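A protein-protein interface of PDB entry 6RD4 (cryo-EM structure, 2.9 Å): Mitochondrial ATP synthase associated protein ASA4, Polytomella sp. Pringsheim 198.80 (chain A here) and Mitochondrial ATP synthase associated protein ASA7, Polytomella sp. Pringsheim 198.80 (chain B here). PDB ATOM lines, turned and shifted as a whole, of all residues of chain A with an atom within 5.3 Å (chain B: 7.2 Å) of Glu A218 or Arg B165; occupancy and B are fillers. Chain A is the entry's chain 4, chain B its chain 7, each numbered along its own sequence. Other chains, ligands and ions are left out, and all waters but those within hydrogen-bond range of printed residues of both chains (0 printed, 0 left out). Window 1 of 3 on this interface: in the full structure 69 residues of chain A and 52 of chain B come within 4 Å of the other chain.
O of Pro B171 sits at hydrogen-bond distance from NH2 of Arg B165 (2.5 Å).
Of the printed residues of chain B, Val A63 touches Arg B165 (3.6 Å) and Pro B171 (3.7 Å). Printed residues of chain B within 4 Å of Val A67: Tyr B161 and Arg B165. Printed residues of chain B within 4 Å of Leu A89: Arg B165 (3.7 Å), His B170 (3.8 Å) and Ala B172 (3.7 Å). Printed residues of chain B within 4 Å of Glu A218: Arg B164 and Arg B165. Of the printed residues of chain A, Tyr B161 touches Val A67, Tyr A85 and Ile A222. Printed residues of chain A within 4 Å of Arg B165: Val A63 (3.6 Å), Val A67 (3.6 Å), Leu A89 (3.7 Å) and Glu A218 (2.6 Å). The nearest residue of chain B that does not touch Glu A218 is Tyr B161 (4.1 Å). The nearest printed residue of chain A that does not touch Arg B164 is Asp A214 (6.3 Å).
Of the 15 printed residues of chain A, 7 touch a printed residue of chain B. Printed residues of chain A that touch a printed residue of chain B: Val A63, Val A67, Tyr A85, Leu A89, Asp A214, Glu A218 and Ile A222. Printed residues of chain B that touch a printed residue of chain A: Tyr B161, Arg B164, Arg B165, His B170, Pro B171, Ala B172 and Gly B174. Hydrophobic or aromatic side chains of chain B within 4 Å of the printed part of chain A: Tyr B161, His B170, Pro B171 and Ala B172. Among the printed residues, Asp or Glu carboxylates within 4 Å of a Lys or Arg side-chain nitrogen of the other chain: Glu A218 with Arg B164 (2.7 Å) and Glu A218 with Arg B165 (2.6 Å).
The side-chain carboxylate (OE1) of Glu A218 is in salt-bridge range of the guanidinium group (NH1) of Arg B164. The side-chain carboxylate (OE1) of Glu A218 lies within salt-bridge range of the guanidinium group (NH1) of Arg B165 (2.6 Å). OH of Tyr B161 sits close to OH of Tyr A85 (2.3 Å).
Among the printed residues, merely in contact across the chains: Val A63 with Arg B165, Val A63 with Pro B171, Val A67 with Tyr B161, Val A67 with Arg B165, Leu A89 with Arg B165, Leu A89 with His B170, Leu A89 with Ala B172, Asp A214 with Gly B174 and Ile A222 with Tyr B161.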
ATOM      1  N   VAL A  63       3.237 -12.268   0.765  1.00  0.00           N
ATOM      2  CA  VAL A  63       1.815 -12.573   0.742  1.00  0.00           C
ATOM      3  C   VAL A  63       1.097 -11.692  -0.268  1.00  0.00           C
ATOM      4  O   VAL A  63       0.258 -12.171  -1.034  1.00  0.00           O
ATOM      5  CB  VAL A  63       1.236 -12.434   2.156  1.00  0.00           C
ATOM      6  CG1 VAL A  63      -0.248 -12.294   2.131  1.00  0.00           C
ATOM      7  CG2 VAL A  63       1.603 -13.622   2.948  1.00  0.00           C
ATOM      8  N   VAL A  67      -1.221 -13.268  -3.134  1.00  0.00           N
ATOM      9  CA  VAL A  67      -2.676 -13.295  -3.057  1.00  0.00           C
ATOM     10  C   VAL A  67      -3.275 -12.915  -4.396  1.00  0.00           C
ATOM     11  O   VAL A  67      -4.283 -13.479  -4.832  1.00  0.00           O
ATOM     12  CB  VAL A  67      -3.131 -12.364  -1.928  1.00  0.00           C
ATOM     13  CG1 VAL A  67      -4.575 -12.014  -2.025  1.00  0.00           C
ATOM     14  CG2 VAL A  67      -2.881 -13.050  -0.659  1.00  0.00           C
ATOM     15  N   LEU A  72      -9.540 -16.822  -7.298  1.00  0.00           N
ATOM     16  CA  LEU A  72     -10.660 -17.180  -6.455  1.00  0.00           C
ATOM     17  C   LEU A  72     -11.564 -18.166  -7.187  1.00  0.00           C
ATOM     18  O   LEU A  72     -11.753 -18.049  -8.395  1.00  0.00           O
ATOM     19  CB  LEU A  72     -11.446 -15.939  -6.101  1.00  0.00           C
ATOM     20  CG  LEU A  72     -11.082 -15.164  -4.866  1.00  0.00           C
ATOM     21  CD1 LEU A  72     -11.633 -13.817  -5.012  1.00  0.00           C
ATOM     22  CD2 LEU A  72     -11.750 -15.820  -3.731  1.00  0.00           C
ATOM     23  N   TYR A  85      -8.071 -23.536  -3.677  1.00  0.00           N
ATOM     24  CA  TYR A  85      -7.896 -22.162  -3.251  1.00  0.00           C
ATOM     25  C   TYR A  85      -7.351 -22.099  -1.851  1.00  0.00           C
ATOM     26  O   TYR A  85      -6.552 -21.220  -1.539  1.00  0.00           O
ATOM     27  CB  TYR A  85      -9.218 -21.429  -3.326  1.00  0.00           C
ATOM     28  CG  TYR A  85      -9.213 -20.110  -2.651  1.00  0.00           C
ATOM     29  CD1 TYR A  85     -10.007 -19.876  -1.569  1.00  0.00           C
ATOM     30  CD2 TYR A  85      -8.410 -19.100  -3.099  1.00  0.00           C
ATOM     31  CE1 TYR A  85     -10.003 -18.679  -0.954  1.00  0.00           C
ATOM     32  CE2 TYR A  85      -8.395 -17.906  -2.491  1.00  0.00           C
ATOM     33  CZ  TYR A  85      -9.193 -17.704  -1.416  1.00  0.00           C
ATOM     34  OH  TYR A  85      -9.195 -16.500  -0.787  1.00  0.00           O
ATOM     35  N   LEU A  89      -3.265 -20.902  -0.539  1.00  0.00           N
ATOM     36  CA  LEU A  89      -3.042 -19.977   0.555  1.00  0.00           C
ATOM     37  C   LEU A  89      -2.270 -20.600   1.698  1.00  0.00           C
ATOM     38  O   LEU A  89      -1.631 -19.876   2.453  1.00  0.00           O
ATOM     39  CB  LEU A  89      -4.370 -19.468   1.087  1.00  0.00           C
ATOM     40  CG  LEU A  89      -5.259 -18.516   0.317  1.00  0.00           C
ATOM     41  CD1 LEU A  89      -6.531 -18.397   1.073  1.00  0.00           C
ATOM     42  CD2 LEU A  89      -4.615 -17.184   0.204  1.00  0.00           C
ATOM     43  N   ASP A 214     -13.652 -22.232   5.811  1.00  0.00           N
ATOM     44  CA  ASP A 214     -13.265 -20.834   5.899  1.00  0.00           C
ATOM     45  C   ASP A 214     -12.958 -20.252   4.539  1.00  0.00           C
ATOM     46  O   ASP A 214     -13.146 -19.055   4.328  1.00  0.00           O
ATOM     47  CB  ASP A 214     -12.035 -20.629   6.767  1.00  0.00           C
ATOM     48  CG  ASP A 214     -12.111 -21.339   8.072  1.00  0.00           C
ATOM     49  OD1 ASP A 214     -11.345 -22.293   8.262  1.00  0.00           O
ATOM     50  OD2 ASP A 214     -12.933 -20.940   8.914  1.00  0.00           O
ATOM     51  N   ALA A 215     -12.433 -21.064   3.630  1.00  0.00           N
ATOM     52  CA  ALA A 215     -12.251 -20.606   2.267  1.00  0.00           C
ATOM     53  C   ALA A 215     -13.583 -20.472   1.567  1.00  0.00           C
ATOM     54  O   ALA A 215     -13.810 -19.498   0.850  1.00  0.00           O
ATOM     55  CB  ALA A 215     -11.346 -21.561   1.509  1.00  0.00           C
ATOM     56  N   ALA A 216     -14.493 -21.417   1.787  1.00  0.00           N
ATOM     57  CA  ALA A 216     -15.787 -21.350   1.127  1.00  0.00           C
ATOM     58  C   ALA A 216     -16.651 -20.252   1.700  1.00  0.00           C
ATOM     59  O   ALA A 216     -17.542 -19.762   1.015  1.00  0.00           O
ATOM     60  CB  ALA A 216     -16.516 -22.681   1.228  1.00  0.00           C
ATOM     61  N   ALA A 217     -16.422 -19.856   2.941  1.00  0.00           N
ATOM     62  CA  ALA A 217     -17.108 -18.690   3.467  1.00  0.00           C
ATOM     63  C   ALA A 217     -16.498 -17.403   2.965  1.00  0.00           C
ATOM     64  O   ALA A 217     -17.148 -16.362   3.024  1.00  0.00           O
ATOM     65  CB  ALA A 217     -17.081 -18.693   4.984  1.00  0.00           C
ATOM     66  N   GLU A 218     -15.251 -17.443   2.517  1.00  0.00           N
ATOM     67  CA  GLU A 218     -14.621 -16.274   1.928  1.00  0.00           C
ATOM     68  C   GLU A 218     -15.038 -16.097   0.486  1.00  0.00           C
ATOM     69  O   GLU A 218     -15.167 -14.971   0.014  1.00  0.00           O
ATOM     70  CB  GLU A 218     -13.106 -16.410   2.025  1.00  0.00           C
ATOM     71  CG  GLU A 218     -12.354 -15.185   1.636  1.00  0.00           C
ATOM     72  CD  GLU A 218     -12.604 -14.036   2.575  1.00  0.00           C
ATOM     73  OE1 GLU A 218     -12.219 -14.155   3.759  1.00  0.00           O
ATOM     74  OE2 GLU A 218     -13.186 -13.019   2.133  1.00  0.00           O
ATOM     75  N   VAL A 219     -15.242 -17.201  -0.219  1.00  0.00           N
ATOM     76  CA  VAL A 219     -15.734 -17.164  -1.586  1.00  0.00           C
ATOM     77  C   VAL A 219     -17.186 -16.730  -1.615  1.00  0.00           C
ATOM     78  O   VAL A 219     -17.576 -15.903  -2.434  1.00  0.00           O
ATOM     79  CB  VAL A 219     -15.531 -18.544  -2.222  1.00  0.00           C
ATOM     80  CG1 VAL A 219     -16.236 -18.657  -3.520  1.00  0.00           C
ATOM     81  CG2 VAL A 219     -14.085 -18.793  -2.384  1.00  0.00           C
ATOM     82  N   LYS A 220     -17.997 -17.224  -0.683  1.00  0.00           N
ATOM     83  CA  LYS A 220     -19.403 -16.842  -0.639  1.00  0.00           C
ATOM     84  C   LYS A 220     -19.616 -15.412  -0.191  1.00  0.00           C
ATOM     85  O   LYS A 220     -20.737 -14.924  -0.275  1.00  0.00           O
ATOM     86  CB  LYS A 220     -20.185 -17.762   0.285  1.00  0.00           C
ATOM     87  CG  LYS A 220     -20.442 -19.129  -0.281  1.00  0.00           C
ATOM     88  CD  LYS A 220     -21.170 -19.067  -1.601  1.00  0.00           C
ATOM     89  CE  LYS A 220     -21.189 -20.427  -2.270  1.00  0.00           C
ATOM     90  NZ  LYS A 220     -22.047 -20.445  -3.477  1.00  0.00           N
ATOM     91  N   ALA A 221     -18.594 -14.740   0.304  1.00  0.00           N
ATOM     92  CA  ALA A 221     -18.713 -13.325   0.589  1.00  0.00           C
ATOM     93  C   ALA A 221     -18.214 -12.460  -0.541  1.00  0.00           C
ATOM     94  O   ALA A 221     -18.630 -11.310  -0.649  1.00  0.00           O
ATOM     95  CB  ALA A 221     -17.941 -12.973   1.845  1.00  0.00           C
ATOM     96  N   ILE A 222     -17.293 -12.967  -1.353  1.00  0.00           N
ATOM     97  CA  ILE A 222     -16.873 -12.255  -2.550  1.00  0.00           C
ATOM     98  C   ILE A 222     -17.924 -12.400  -3.631  1.00  0.00           C
ATOM     99  O   ILE A 222     -18.189 -11.468  -4.389  1.00  0.00           O
ATOM    100  CB  ILE A 222     -15.497 -12.770  -3.010  1.00  0.00           C
ATOM    101  CG1 ILE A 222     -14.443 -12.451  -1.973  1.00  0.00           C
ATOM    102  CG2 ILE A 222     -15.071 -12.145  -4.283  1.00  0.00           C
ATOM    103  CD1 ILE A 222     -14.329 -11.000  -1.674  1.00  0.00           C
ATOM    104  N   GLU A 223     -18.561 -13.563  -3.696  1.00  0.00           N
ATOM    105  CA  GLU A 223     -19.675 -13.766  -4.606  1.00  0.00           C
ATOM    106  C   GLU A 223     -20.846 -12.873  -4.253  1.00  0.00           C
ATOM    107  O   GLU A 223     -21.536 -12.371  -5.138  1.00  0.00           O
ATOM    108  CB  GLU A 223     -20.121 -15.212  -4.556  1.00  0.00           C
ATOM    109  CG  GLU A 223     -19.235 -16.159  -5.253  1.00  0.00           C
ATOM    110  CD  GLU A 223     -19.793 -17.537  -5.220  1.00  0.00           C
ATOM    111  OE1 GLU A 223     -20.940 -17.683  -4.779  1.00  0.00           O
ATOM    112  OE2 GLU A 223     -19.103 -18.481  -5.635  1.00  0.00           O
ATOM    113  N   ASN B 160     -10.394  -4.809  -0.678  1.00  0.00           N
ATOM    114  CA  ASN B 160     -10.910  -5.262   0.603  1.00  0.00           C
ATOM    115  C   ASN B 160     -10.660  -6.737   0.824  1.00  0.00           C
ATOM    116  O   ASN B 160     -10.506  -7.166   1.967  1.00  0.00           O
ATOM    117  CB  ASN B 160     -12.402  -4.984   0.700  1.00  0.00           C
ATOM    118  CG  ASN B 160     -12.698  -3.593   1.165  1.00  0.00           C
ATOM    119  OD1 ASN B 160     -11.881  -2.963   1.825  1.00  0.00           O
ATOM    120  ND2 ASN B 160     -13.872  -3.100   0.831  1.00  0.00           N
ATOM    121  N   TYR B 161     -10.647  -7.531  -0.245  1.00  0.00           N
ATOM    122  CA  TYR B 161     -10.282  -8.934  -0.121  1.00  0.00           C
ATOM    123  C   TYR B 161      -8.812  -9.071   0.204  1.00  0.00           C
ATOM    124  O   TYR B 161      -8.430  -9.893   1.036  1.00  0.00           O
ATOM    125  CB  TYR B 161     -10.603  -9.681  -1.413  1.00  0.00           C
ATOM    126  CG  TYR B 161      -9.958 -11.036  -1.536  1.00  0.00           C
ATOM    127  CD1 TYR B 161      -8.802 -11.213  -2.271  1.00  0.00           C
ATOM    128  CD2 TYR B 161     -10.519 -12.141  -0.952  1.00  0.00           C
ATOM    129  CE1 TYR B 161      -8.214 -12.424  -2.369  1.00  0.00           C
ATOM    130  CE2 TYR B 161      -9.939 -13.364  -1.072  1.00  0.00           C
ATOM    131  CZ  TYR B 161      -8.787 -13.493  -1.778  1.00  0.00           C
ATOM    132  OH  TYR B 161      -8.190 -14.710  -1.914  1.00  0.00           O
ATOM    133  N   ALA B 162      -7.973  -8.288  -0.460  1.00  0.00           N
ATOM    134  CA  ALA B 162      -6.539  -8.411  -0.287  1.00  0.00           C
ATOM    135  C   ALA B 162      -6.075  -7.953   1.080  1.00  0.00           C
ATOM    136  O   ALA B 162      -5.006  -8.371   1.516  1.00  0.00           O
ATOM    137  CB  ALA B 162      -5.818  -7.618  -1.361  1.00  0.00           C
ATOM    138  N   ALA B 163      -6.848  -7.118   1.764  1.00  0.00           N
ATOM    139  CA  ALA B 163      -6.503  -6.715   3.117  1.00  0.00           C
ATOM    140  C   ALA B 163      -6.906  -7.755   4.140  1.00  0.00           C
ATOM    141  O   ALA B 163      -6.308  -7.823   5.210  1.00  0.00           O
ATOM    142  CB  ALA B 163      -7.157  -5.386   3.446  1.00  0.00           C
ATOM    143  N   ARG B 164      -7.915  -8.564   3.844  1.00  0.00           N
ATOM    144  CA  ARG B 164      -8.245  -9.671   4.726  1.00  0.00           C
ATOM    145  C   ARG B 164      -7.229 -10.781   4.617  1.00  0.00           C
ATOM    146  O   ARG B 164      -7.111 -11.604   5.525  1.00  0.00           O
ATOM    147  CB  ARG B 164      -9.622 -10.210   4.404  1.00  0.00           C
ATOM    148  CG  ARG B 164     -10.717  -9.292   4.797  1.00  0.00           C
ATOM    149  CD  ARG B 164     -12.036  -9.898   4.458  1.00  0.00           C
ATOM    150  NE  ARG B 164     -12.075 -11.303   4.812  1.00  0.00           N
ATOM    151  CZ  ARG B 164     -12.442 -11.749   6.001  1.00  0.00           C
ATOM    152  NH1 ARG B 164     -12.451 -13.045   6.244  1.00  0.00           N
ATOM    153  NH2 ARG B 164     -12.796 -10.898   6.945  1.00  0.00           N
ATOM    154  N   ARG B 165      -6.509 -10.840   3.507  1.00  0.00           N
ATOM    155  CA  ARG B 165      -5.458 -11.821   3.351  1.00  0.00           C
ATOM    156  C   ARG B 165      -4.153 -11.360   3.957  1.00  0.00           C
ATOM    157  O   ARG B 165      -3.267 -12.180   4.176  1.00  0.00           O
ATOM    158  CB  ARG B 165      -5.232 -12.129   1.886  1.00  0.00           C
ATOM    159  CG  ARG B 165      -6.315 -12.878   1.189  1.00  0.00           C
ATOM    160  CD  ARG B 165      -6.672 -14.107   1.897  1.00  0.00           C
ATOM    161  NE  ARG B 165      -7.951 -13.924   2.534  1.00  0.00           N
ATOM    162  CZ  ARG B 165      -8.531 -14.829   3.292  1.00  0.00           C
ATOM    163  NH1 ARG B 165      -9.698 -14.573   3.840  1.00  0.00           N
ATOM    164  NH2 ARG B 165      -7.939 -15.985   3.499  1.00  0.00           N
ATOM    165  N   ARG B 166      -4.014 -10.075   4.242  1.00  0.00           N
ATOM    166  CA  ARG B 166      -2.865  -9.569   4.981  1.00  0.00           C
ATOM    167  C   ARG B 166      -3.107  -9.663   6.470  1.00  0.00           C
ATOM    168  O   ARG B 166      -2.975  -8.702   7.206  1.00  0.00           O
ATOM    169  CB  ARG B 166      -2.565  -8.140   4.576  1.00  0.00           C
ATOM    170  CG  ARG B 166      -1.696  -8.036   3.374  1.00  0.00           C
ATOM    171  CD  ARG B 166      -1.175  -6.641   3.239  1.00  0.00           C
ATOM    172  NE  ARG B 166      -2.229  -5.653   3.389  1.00  0.00           N
ATOM    173  CZ  ARG B 166      -3.002  -5.232   2.401  1.00  0.00           C
ATOM    174  NH1 ARG B 166      -3.932  -4.327   2.627  1.00  0.00           N
ATOM    175  NH2 ARG B 166      -2.847  -5.713   1.189  1.00  0.00           N
ATOM    176  N   SER B 167      -3.469 -10.851   6.919  1.00  0.00           N
ATOM    177  CA  SER B 167      -3.751 -11.076   8.314  1.00  0.00           C
ATOM    178  C   SER B 167      -2.441 -11.233   9.052  1.00  0.00           C
ATOM    179  O   SER B 167      -1.449 -11.691   8.495  1.00  0.00           O
ATOM    180  CB  SER B 167      -4.615 -12.317   8.474  1.00  0.00           C
ATOM    181  OG  SER B 167      -4.992 -12.518   9.814  1.00  0.00           O
ATOM    182  N   THR B 168      -2.434 -10.822  10.307  1.00  0.00           N
ATOM    183  CA  THR B 168      -1.253 -10.970  11.134  1.00  0.00           C
ATOM    184  C   THR B 168      -1.099 -12.374  11.682  1.00  0.00           C
ATOM    185  O   THR B 168      -0.102 -12.656  12.347  1.00  0.00           O
ATOM    186  CB  THR B 168      -1.310  -9.987  12.289  1.00  0.00           C
ATOM    187  OG1 THR B 168      -2.461 -10.271  13.086  1.00  0.00           O
ATOM    188  CG2 THR B 168      -1.416  -8.591  11.765  1.00  0.00           C
ATOM    189  N   HIS B 170      -2.313 -15.569   9.672  1.00  0.00           N
ATOM    190  CA  HIS B 170      -2.028 -16.403   8.514  1.00  0.00           C
ATOM    191  C   HIS B 170      -2.892 -15.917   7.368  1.00  0.00           C
ATOM    192  O   HIS B 170      -3.977 -15.387   7.613  1.00  0.00           O
ATOM    193  CB  HIS B 170      -2.316 -17.879   8.806  1.00  0.00           C
ATOM    194  CG  HIS B 170      -1.686 -18.825   7.838  1.00  0.00           C
ATOM    195  ND1 HIS B 170      -0.461 -19.402   8.051  1.00  0.00           N
ATOM    196  CD2 HIS B 170      -2.121 -19.306   6.656  1.00  0.00           C
ATOM    197  CE1 HIS B 170      -0.164 -20.186   7.033  1.00  0.00           C
ATOM    198  NE2 HIS B 170      -1.155 -20.143   6.172  1.00  0.00           N
ATOM    199  N   PRO B 171      -2.441 -16.054   6.119  1.00  0.00           N
ATOM    200  CA  PRO B 171      -3.322 -15.745   4.985  1.00  0.00           C
ATOM    201  C   PRO B 171      -4.559 -16.609   4.893  1.00  0.00           C
ATOM    202  O   PRO B 171      -5.602 -16.126   4.456  1.00  0.00           O
ATOM    203  CB  PRO B 171      -2.411 -15.978   3.785  1.00  0.00           C
ATOM    204  CG  PRO B 171      -1.092 -15.755   4.287  1.00  0.00           C
ATOM    205  CD  PRO B 171      -1.042 -16.146   5.696  1.00  0.00           C
ATOM    206  N   ALA B 172      -4.476 -17.870   5.300  1.00  0.00           N
ATOM    207  CA  ALA B 172      -5.541 -18.843   5.161  1.00  0.00           C
ATOM    208  C   ALA B 172      -6.307 -19.072   6.444  1.00  0.00           C
ATOM    209  O   ALA B 172      -7.000 -20.082   6.563  1.00  0.00           O
ATOM    210  CB  ALA B 172      -4.976 -20.169   4.677  1.00  0.00           C
ATOM    211  N   ILE B 173      -6.201 -18.188   7.398  1.00  0.00           N
ATOM    212  CA  ILE B 173      -6.875 -18.394   8.669  1.00  0.00           C
ATOM    213  C   ILE B 173      -8.355 -18.082   8.506  1.00  0.00           C
ATOM    214  O   ILE B 173      -8.760 -17.311   7.633  1.00  0.00           O
ATOM    215  CB  ILE B 173      -6.207 -17.547   9.772  1.00  0.00           C
ATOM    216  CG1 ILE B 173      -6.488 -18.114  11.159  1.00  0.00           C
ATOM    217  CG2 ILE B 173      -6.603 -16.096   9.684  1.00  0.00           C
ATOM    218  CD1 ILE B 173      -6.115 -19.529  11.328  1.00  0.00           C
ATOM    219  N   GLY B 174      -9.181 -18.745   9.305  1.00  0.00           N
ATOM    220  CA  GLY B 174     -10.598 -18.464   9.337  1.00  0.00           C
ATOM    221  C   GLY B 174     -11.144 -18.735  10.718  1.00  0.00           C
ATOM    222  O   GLY B 174     -10.398 -19.055  11.632  1.00  0.00           O
